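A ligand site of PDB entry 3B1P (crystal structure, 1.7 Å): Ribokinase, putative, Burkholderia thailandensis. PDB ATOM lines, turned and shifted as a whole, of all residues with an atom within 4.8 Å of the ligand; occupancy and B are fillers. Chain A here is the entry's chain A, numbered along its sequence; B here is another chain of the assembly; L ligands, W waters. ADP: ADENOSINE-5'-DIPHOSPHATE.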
ATOM      1  N   ASN A 111      26.845  13.488 -19.509  1.00  0.00           N
ATOM      2  CA  ASN A 111      26.087  14.666 -19.866  1.00  0.00           C
ATOM      3  C   ASN A 111      26.919  15.914 -20.127  1.00  0.00           C
ATOM      4  O   ASN A 111      26.475  17.058 -19.949  1.00  0.00           O
ATOM      5  CB  ASN A 111      24.986  14.939 -18.779  1.00  0.00           C
ATOM      6  CG  ASN A 111      23.729  15.613 -19.339  1.00  0.00           C
ATOM      7  OD1 ASN A 111      23.560  15.815 -20.566  1.00  0.00           O
ATOM      8  ND2 ASN A 111      22.830  15.963 -18.424  1.00  0.00           N
ATOM      9  N   ASN A 192      23.251  23.206 -13.204  1.00  0.00           N
ATOM     10  CA  ASN A 192      24.151  22.084 -12.878  1.00  0.00           C
ATOM     11  C   ASN A 192      25.480  22.616 -12.314  1.00  0.00           C
ATOM     12  O   ASN A 192      25.693  23.839 -12.279  1.00  0.00           O
ATOM     13  CB  ASN A 192      24.319  21.088 -14.066  1.00  0.00           C
ATOM     14  CG  ASN A 192      25.196  21.620 -15.212  1.00  0.00           C
ATOM     15  OD1 ASN A 192      26.014  22.534 -15.051  1.00  0.00           O
ATOM     16  ND2 ASN A 192      25.054  20.981 -16.383  1.00  0.00           N
ATOM     17  N   GLU A 195      27.491  24.938 -14.712  1.00  0.00           N
ATOM     18  CA  GLU A 195      26.792  26.243 -14.822  1.00  0.00           C
ATOM     19  C   GLU A 195      26.932  27.050 -13.557  1.00  0.00           C
ATOM     20  O   GLU A 195      27.078  28.266 -13.625  1.00  0.00           O
ATOM     21  CB  GLU A 195      25.301  26.020 -15.089  1.00  0.00           C
ATOM     22  CG  GLU A 195      25.114  25.374 -16.479  1.00  0.00           C
ATOM     23  CD  GLU A 195      23.813  24.635 -16.660  1.00  0.00           C
ATOM     24  OE1 GLU A 195      23.005  24.486 -15.719  1.00  0.00           O
ATOM     25  OE2 GLU A 195      23.624  24.218 -17.813  1.00  0.00           O
ATOM     26  N   THR A 220      22.653  20.821  -9.511  1.00  0.00           N
ATOM     27  CA  THR A 220      22.630  19.388  -9.838  1.00  0.00           C
ATOM     28  C   THR A 220      24.019  18.869 -10.217  1.00  0.00           C
ATOM     29  O   THR A 220      24.818  19.591 -10.815  1.00  0.00           O
ATOM     30  CB  THR A 220      21.637  19.026 -10.929  1.00  0.00           C
ATOM     31  OG1 THR A 220      22.020  19.558 -12.189  1.00  0.00           O
ATOM     32  CG2 THR A 220      20.213  19.546 -10.599  1.00  0.00           C
ATOM     33  N   ARG A 221      24.247  17.603  -9.876  1.00  0.00           N
ATOM     34  CA  ARG A 221      25.551  16.963  -9.996  1.00  0.00           C
ATOM     35  C   ARG A 221      25.487  15.602 -10.664  1.00  0.00           C
ATOM     36  O   ARG A 221      26.229  14.679 -10.295  1.00  0.00           O
ATOM     37  CB  ARG A 221      26.219  16.877  -8.604  1.00  0.00           C
ATOM     38  CG  ARG A 221      26.153  18.214  -7.881  1.00  0.00           C
ATOM     39  CD  ARG A 221      26.616  18.136  -6.407  1.00  0.00           C
ATOM     40  NE  ARG A 221      26.332  19.405  -5.704  1.00  0.00           N
ATOM     41  CZ  ARG A 221      27.124  20.475  -5.771  1.00  0.00           C
ATOM     42  NH1 ARG A 221      28.196  20.429  -6.565  1.00  0.00           N
ATOM     43  NH2 ARG A 221      26.842  21.572  -5.064  1.00  0.00           N
ATOM     44  N   GLY A 222      24.638  15.470 -11.697  1.00  0.00           N
ATOM     45  CA  GLY A 222      24.550  14.237 -12.467  1.00  0.00           C
ATOM     46  C   GLY A 222      24.258  12.990 -11.625  1.00  0.00           C
ATOM     47  O   GLY A 222      23.368  13.039 -10.740  1.00  0.00           O
ATOM     48  N   GLU A 223      25.075  11.958 -11.795  1.00  0.00           N
ATOM     49  CA  GLU A 223      24.888  10.714 -11.053  1.00  0.00           C
ATOM     50  C   GLU A 223      25.126  10.874  -9.546  1.00  0.00           C
ATOM     51  O   GLU A 223      24.763   9.984  -8.746  1.00  0.00           O
ATOM     52  CB  GLU A 223      25.772   9.580 -11.645  1.00  0.00           C
ATOM     53  CG  GLU A 223      27.245   9.671 -11.237  1.00  0.00           C
ATOM     54  CD  GLU A 223      28.113   8.597 -11.904  1.00  0.00           C
ATOM     55  OE1 GLU A 223      27.564   7.507 -12.215  1.00  0.00           O
ATOM     56  OE2 GLU A 223      29.319   8.852 -12.129  1.00  0.00           O
ATOM     57  N   GLY A 225      23.618  13.167  -7.753  1.00  0.00           N
ATOM     58  CA  GLY A 225      22.404  13.751  -7.147  1.00  0.00           C
ATOM     59  C   GLY A 225      22.424  15.274  -7.240  1.00  0.00           C
ATOM     60  O   GLY A 225      22.728  15.825  -8.304  1.00  0.00           O
ATOM     61  N   ALA A 226      22.070  15.971  -6.146  1.00  0.00           N
ATOM     62  CA  ALA A 226      21.949  17.413  -6.181  1.00  0.00           C
ATOM     63  C   ALA A 226      22.074  18.008  -4.782  1.00  0.00           C
ATOM     64  O   ALA A 226      21.991  17.293  -3.784  1.00  0.00           O
ATOM     65  CB  ALA A 226      20.563  17.854  -6.801  1.00  0.00           C
ATOM     66  N   ALA A 239      20.995  10.765  -5.762  1.00  0.00           N
ATOM     67  CA  ALA A 239      20.491  10.270  -7.037  1.00  0.00           C
ATOM     68  C   ALA A 239      19.670   9.013  -6.826  1.00  0.00           C
ATOM     69  O   ALA A 239      19.887   8.261  -5.831  1.00  0.00           O
ATOM     70  CB  ALA A 239      21.666   9.941  -8.007  1.00  0.00           C
ATOM     71  N   VAL A 240      18.732   8.770  -7.748  1.00  0.00           N
ATOM     72  CA  VAL A 240      18.075   7.463  -7.865  1.00  0.00           C
ATOM     73  C   VAL A 240      18.852   6.634  -8.888  1.00  0.00           C
ATOM     74  O   VAL A 240      19.202   7.130  -9.961  1.00  0.00           O
ATOM     75  CB  VAL A 240      16.609   7.580  -8.319  1.00  0.00           C
ATOM     76  CG1 VAL A 240      15.953   6.193  -8.565  1.00  0.00           C
ATOM     77  CG2 VAL A 240      15.764   8.446  -7.360  1.00  0.00           C
ATOM     78  N   ALA A 242      19.748   4.632 -11.872  1.00  0.00           N
ATOM     79  CA  ALA A 242      19.039   4.497 -13.146  1.00  0.00           C
ATOM     80  C   ALA A 242      18.890   3.023 -13.515  1.00  0.00           C
ATOM     81  O   ALA A 242      19.813   2.239 -13.261  1.00  0.00           O
ATOM     82  CB  ALA A 242      19.837   5.245 -14.242  1.00  0.00           C
ATOM     83  N   VAL A 245      21.588   3.527 -18.310  1.00  0.00           N
ATOM     84  CA  VAL A 245      22.053   4.868 -18.678  1.00  0.00           C
ATOM     85  C   VAL A 245      22.117   4.905 -20.214  1.00  0.00           C
ATOM     86  O   VAL A 245      22.976   4.236 -20.836  1.00  0.00           O
ATOM     87  CB  VAL A 245      23.390   5.237 -17.979  1.00  0.00           C
ATOM     88  CG1 VAL A 245      23.916   6.580 -18.472  1.00  0.00           C
ATOM     89  CG2 VAL A 245      23.188   5.319 -16.476  1.00  0.00           C
ATOM     90  N   PRO A 248      21.645  11.144 -21.271  1.00  0.00           N
ATOM     91  CA  PRO A 248      21.380  12.107 -20.222  1.00  0.00           C
ATOM     92  C   PRO A 248      20.806  13.428 -20.754  1.00  0.00           C
ATOM     93  O   PRO A 248      20.494  14.290 -19.965  1.00  0.00           O
ATOM     94  CB  PRO A 248      22.781  12.359 -19.625  1.00  0.00           C
ATOM     95  CG  PRO A 248      23.660  12.257 -20.893  1.00  0.00           C
ATOM     96  CD  PRO A 248      23.103  10.998 -21.509  1.00  0.00           C
ATOM     97  N   GLY A 250      18.654  16.372 -21.334  1.00  0.00           N
ATOM     98  CA  GLY A 250      17.412  16.823 -20.714  1.00  0.00           C
ATOM     99  C   GLY A 250      17.165  16.223 -19.340  1.00  0.00           C
ATOM    100  O   GLY A 250      16.055  16.415 -18.828  1.00  0.00           O
ATOM    101  N   CYS A 251      18.164  15.546 -18.743  1.00  0.00           N
ATOM    102  CA  CYS A 251      18.015  15.140 -17.291  1.00  0.00           C
ATOM    103  C   CYS A 251      17.700  16.349 -16.456  1.00  0.00           C
ATOM    104  O   CYS A 251      16.813  16.259 -15.585  1.00  0.00           O
ATOM    105  CB  CYS A 251      19.239  14.399 -16.760  1.00  0.00           C
ATOM    106  SG  CYS A 251      19.282  12.708 -17.258  1.00  0.00           S
ATOM    107  N   GLY A 252      18.442  17.460 -16.631  1.00  0.00           N
ATOM    108  CA  GLY A 252      18.201  18.636 -15.793  1.00  0.00           C
ATOM    109  C   GLY A 252      16.792  19.159 -16.002  1.00  0.00           C
ATOM    110  O   GLY A 252      16.174  19.692 -15.081  1.00  0.00           O
ATOM    111  N   PHE A 255      14.361  17.000 -14.149  1.00  0.00           N
ATOM    112  CA  PHE A 255      14.543  17.395 -12.754  1.00  0.00           C
ATOM    113  C   PHE A 255      13.784  18.704 -12.463  1.00  0.00           C
ATOM    114  O   PHE A 255      13.065  18.837 -11.486  1.00  0.00           O
ATOM    115  CB  PHE A 255      16.075  17.576 -12.506  1.00  0.00           C
ATOM    116  CG  PHE A 255      16.460  17.932 -11.091  1.00  0.00           C
ATOM    117  CD1 PHE A 255      16.906  16.943 -10.242  1.00  0.00           C
ATOM    118  CD2 PHE A 255      16.383  19.251 -10.630  1.00  0.00           C
ATOM    119  CE1 PHE A 255      17.323  17.280  -8.882  1.00  0.00           C
ATOM    120  CE2 PHE A 255      16.744  19.598  -9.314  1.00  0.00           C
ATOM    121  CZ  PHE A 255      17.208  18.603  -8.454  1.00  0.00           C
ATOM    122  N   ARG A 256      13.916  19.712 -13.334  1.00  0.00           N
ATOM    123  CA  ARG A 256      13.218  20.974 -13.081  1.00  0.00           C
ATOM    124  C   ARG A 256      11.668  20.839 -13.083  1.00  0.00           C
ATOM    125  O   ARG A 256      11.012  21.547 -12.367  1.00  0.00           O
ATOM    126  CB  ARG A 256      13.623  21.991 -14.155  1.00  0.00           C
ATOM    127  CG  ARG A 256      14.977  22.642 -13.724  1.00  0.00           C
ATOM    128  CD  ARG A 256      15.757  23.052 -14.943  1.00  0.00           C
ATOM    129  NE  ARG A 256      17.091  23.577 -14.618  1.00  0.00           N
ATOM    130  CZ  ARG A 256      18.135  22.873 -14.156  1.00  0.00           C
ATOM    131  NH1 ARG A 256      18.019  21.578 -13.833  1.00  0.00           N
ATOM    132  NH2 ARG A 256      19.328  23.468 -13.981  1.00  0.00           N
ATOM    133  N   SER A 277      15.024  14.428  -8.549  1.00  0.00           N
ATOM    134  CA  SER A 277      16.090  13.480  -8.755  1.00  0.00           C
ATOM    135  C   SER A 277      15.566  12.196  -9.413  1.00  0.00           C
ATOM    136  O   SER A 277      16.148  11.650 -10.381  1.00  0.00           O
ATOM    137  CB  SER A 277      16.789  13.200  -7.385  1.00  0.00           C
ATOM    138  OG  SER A 277      17.811  12.258  -7.578  1.00  0.00           O
ATOM    139  N   GLY A 280      14.846  12.806 -13.211  1.00  0.00           N
ATOM    140  CA  GLY A 280      16.103  12.722 -13.984  1.00  0.00           C
ATOM    141  C   GLY A 280      16.524  11.282 -14.217  1.00  0.00           C
ATOM    142  O   GLY A 280      16.966  10.930 -15.281  1.00  0.00           O
ATOM    143  N   ALA A 281      16.396  10.417 -13.187  1.00  0.00           N
ATOM    144  CA  ALA A 281      16.727   8.981 -13.350  1.00  0.00           C
ATOM    145  C   ALA A 281      15.758   8.235 -14.283  1.00  0.00           C
ATOM    146  O   ALA A 281      16.191   7.345 -15.017  1.00  0.00           O
ATOM    147  CB  ALA A 281      16.773   8.266 -11.978  1.00  0.00           C
ATOM    148  N   ILE A 284      16.803   9.304 -17.947  1.00  0.00           N
ATOM    149  CA  ILE A 284      18.108   8.855 -18.489  1.00  0.00           C
ATOM    150  C   ILE A 284      18.053   7.455 -19.051  1.00  0.00           C
ATOM    151  O   ILE A 284      18.912   7.065 -19.841  1.00  0.00           O
ATOM    152  CB  ILE A 284      19.242   9.002 -17.423  1.00  0.00           C
ATOM    153  CG1 ILE A 284      20.641   9.074 -18.113  1.00  0.00           C
ATOM    154  CG2 ILE A 284      19.169   7.799 -16.449  1.00  0.00           C
ATOM    155  CD1 ILE A 284      21.753   9.498 -17.153  1.00  0.00           C
ATOM    156  N   HIS B  31      30.272  17.728 -14.505  1.00  0.00           N
ATOM    157  CA  HIS B  31      30.162  18.071 -15.927  1.00  0.00           C
ATOM    158  C   HIS B  31      31.365  18.908 -16.284  1.00  0.00           C
ATOM    159  O   HIS B  31      31.497  19.994 -15.800  1.00  0.00           O
ATOM    160  CB  HIS B  31      28.928  18.917 -16.198  1.00  0.00           C
ATOM    161  CG  HIS B  31      27.660  18.272 -15.718  1.00  0.00           C
ATOM    162  ND1 HIS B  31      27.230  18.384 -14.419  1.00  0.00           N
ATOM    163  CD2 HIS B  31      26.688  17.600 -16.396  1.00  0.00           C
ATOM    164  CE1 HIS B  31      26.066  17.749 -14.286  1.00  0.00           C
ATOM    165  NE2 HIS B  31      25.724  17.250 -15.478  1.00  0.00           N
ATOM    166  N   ASN B  34      29.921  22.151 -20.784  1.00  0.00           N
ATOM    167  CA  ASN B  34      28.590  22.372 -21.362  1.00  0.00           C
ATOM    168  C   ASN B  34      28.748  23.581 -22.266  1.00  0.00           C
ATOM    169  O   ASN B  34      29.165  24.679 -21.804  1.00  0.00           O
ATOM    170  CB  ASN B  34      27.643  22.852 -20.266  1.00  0.00           C
ATOM    171  CG  ASN B  34      27.007  21.755 -19.489  1.00  0.00           C
ATOM    172  OD1 ASN B  34      27.253  20.560 -19.668  1.00  0.00           O
ATOM    173  ND2 ASN B  34      26.147  22.171 -18.590  1.00  0.00           N
HETATM  174  PB  ADP L   1      21.795  18.776 -16.639  1.00  0.00           P
HETATM  175  O1B ADP L   1      20.979  18.013 -17.645  1.00  0.00           O
HETATM  176  O2B ADP L   1      23.295  18.839 -16.940  1.00  0.00           O
HETATM  177  O3B ADP L   1      21.273  20.105 -16.340  1.00  0.00           O
HETATM  178  PA  ADP L   1      22.379  16.811 -14.516  1.00  0.00           P
HETATM  179  O1A ADP L   1      23.282  15.993 -15.424  1.00  0.00           O
HETATM  180  O2A ADP L   1      23.053  17.335 -13.253  1.00  0.00           O
HETATM  181  O3A ADP L   1      21.606  17.998 -15.231  1.00  0.00           O
HETATM  182  O5' ADP L   1      21.186  15.776 -14.173  1.00  0.00           O
HETATM  183  C5' ADP L   1      20.109  16.294 -13.399  1.00  0.00           C
HETATM  184  C4' ADP L   1      19.635  15.209 -12.405  1.00  0.00           C
HETATM  185  O4' ADP L   1      19.270  14.037 -13.142  1.00  0.00           O
HETATM  186  C3' ADP L   1      20.679  14.724 -11.445  1.00  0.00           C
HETATM  187  O3' ADP L   1      20.814  15.600 -10.321  1.00  0.00           O
HETATM  188  C2' ADP L   1      20.178  13.324 -11.134  1.00  0.00           C
HETATM  189  O2' ADP L   1      19.173  13.502 -10.099  1.00  0.00           O
HETATM  190  C1' ADP L   1      19.576  12.828 -12.454  1.00  0.00           C
HETATM  191  N9  ADP L   1      20.674  12.153 -13.175  1.00  0.00           N
HETATM  192  C8  ADP L   1      21.581  12.683 -14.073  1.00  0.00           C
HETATM  193  N7  ADP L   1      22.508  11.736 -14.411  1.00  0.00           N
HETATM  194  C5  ADP L   1      22.141  10.562 -13.755  1.00  0.00           C
HETATM  195  C6  ADP L   1      22.655   9.168 -13.654  1.00  0.00           C
HETATM  196  N6  ADP L   1      23.758   8.802 -14.374  1.00  0.00           N
HETATM  197  N1  ADP L   1      21.997   8.302 -12.843  1.00  0.00           N
HETATM  198  C2  ADP L   1      20.894   8.686 -12.138  1.00  0.00           C
HETATM  199  N3  ADP L   1      20.382   9.922 -12.154  1.00  0.00           N
HETATM  200  C4  ADP L   1      20.962  10.870 -12.944  1.00  0.00           C
HETATM  201  O   HOH W   1      21.754  22.176 -17.974  1.00  0.00           O
HETATM  202  O   HOH W   2      19.427  14.781  -7.563  1.00  0.00           O
HETATM  203  O   HOH W   3      20.786  17.840 -20.335  1.00  0.00           O
HETATM  204  O   HOH W   4      22.400   5.842 -11.940  1.00  0.00           O
HETATM  205  O   HOH W   5      25.647  10.369 -16.050  1.00  0.00           O
HETATM  206  O   HOH W   6      25.615   6.647 -14.170  1.00  0.00           O
HETATM  207  O   HOH W   7      18.721  10.641  -9.890  1.00  0.00           O
HETATM  208  O   HOH W   8      24.630  18.926 -19.140  1.00  0.00           O
HETATM  209  O   HOH W   9      24.078  13.351 -16.109  1.00  0.00           O
HETATM  210  O   HOH W  10      20.562  21.004 -13.859  1.00  0.00           O
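Water W8 lies within hydrogen-bond range of O2B of the ligand, O of Asn 111, OD1 of Asn 34 of chain B and ND2 of Asn 192.
Water W4 lies within hydrogen-bond range of a nitrogen (N1) of the ligand (2.7 Å) and the backbone NH (N) of Ala 242 (2.9 Å).
Water W10 lies within hydrogen-bond range of the guanidinium group (NH1) of Arg 256 (2.6 Å), the side-chain hydroxyl (OG1) of Thr 220 (2.6 Å) and an oxygen (O3B) of the ligand (2.7 Å).
Water W2 lies within hydrogen-bond range of an oxygen (O2') of the ligand (2.9 Å), the side-chain hydroxyl of Ser 277 (3.0 Å) and the backbone NH of Ala 226 (3.2 Å).
Water W6 lies within hydrogen-bond range of a nitrogen (N6) of the ligand and the side-chain carboxylate (OE1) of Glu 223.
Water W7 lies within hydrogen-bond range of the backbone carbonyl oxygen of Ser 277 (2.8 Å), the backbone NH of Val 240 (2.8 Å) and a nitrogen (N3) of the ligand (2.9 Å).
N of Arg 221 touches O2A of the ligand (3.6 Å).
CB of Glu 223 touches N6 of the ligand, 3.5 Å away.
O of Val 240 touches C2 of the ligand (3.2 Å).
Ala 242 touches the ligand (CB to N1, 3.996 Å).
Cys 251 touches the ligand (CB to O5', 3.5 Å).
Phe 255 touches the ligand (CD1 to C4', 3.9 Å).
Gly 280 touches the ligand.
CA of Ala 281 touches N3 of the ligand (3.96 Å).
Ile 284 touches the ligand (CD1 to N6, 3.5 Å).
N of Gly 222 sits at hydrogen-bond distance from O2A of the ligand, at 2.9 Å.
The side-chain hydroxyl of Ser 277 lies within hydrogen-bond range of an oxygen (O2') of the ligand.
ND2 of Asn 111 is in hydrogen-bond range of O1B of the ligand.
O2B of the ligand is in hydrogen-bond range of ND2 of Asn 192 (2.8 Å).
O2A of the ligand sits at hydrogen-bond distance from OG1 of Thr 220 (2.7 Å).
NE2 of His 31 of chain B sits at hydrogen-bond distance from O1A of the ligand (2.7 Å).
N of Gly 252 is in hydrogen-bond range of O1B of the ligand.
O of Gly 225 lies within hydrogen-bond range of O3' of the ligand (2.8 Å).
ND2 of Asn 192 lies close to ND2 of Asn 34 of chain B, 2.7 Å away.
NH1 of Arg 256 sits at hydrogen-bond distance from O of Gly 252, at 2.9 Å.
N of Asn 192 is in hydrogen-bond range of OE1 of Glu 195.
The side-chain sulfur (SG) of Cys 251 sits at hydrogen-bond distance from the backbone carbonyl oxygen (O) of Pro 248, 3.4 Å away.
SG of Cys 251 sits at hydrogen-bond distance from O of Gly 280 (3.5 Å).
ND2 of Asn 111 lies within hydrogen-bond range of O of Pro 248 (3.3 Å).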
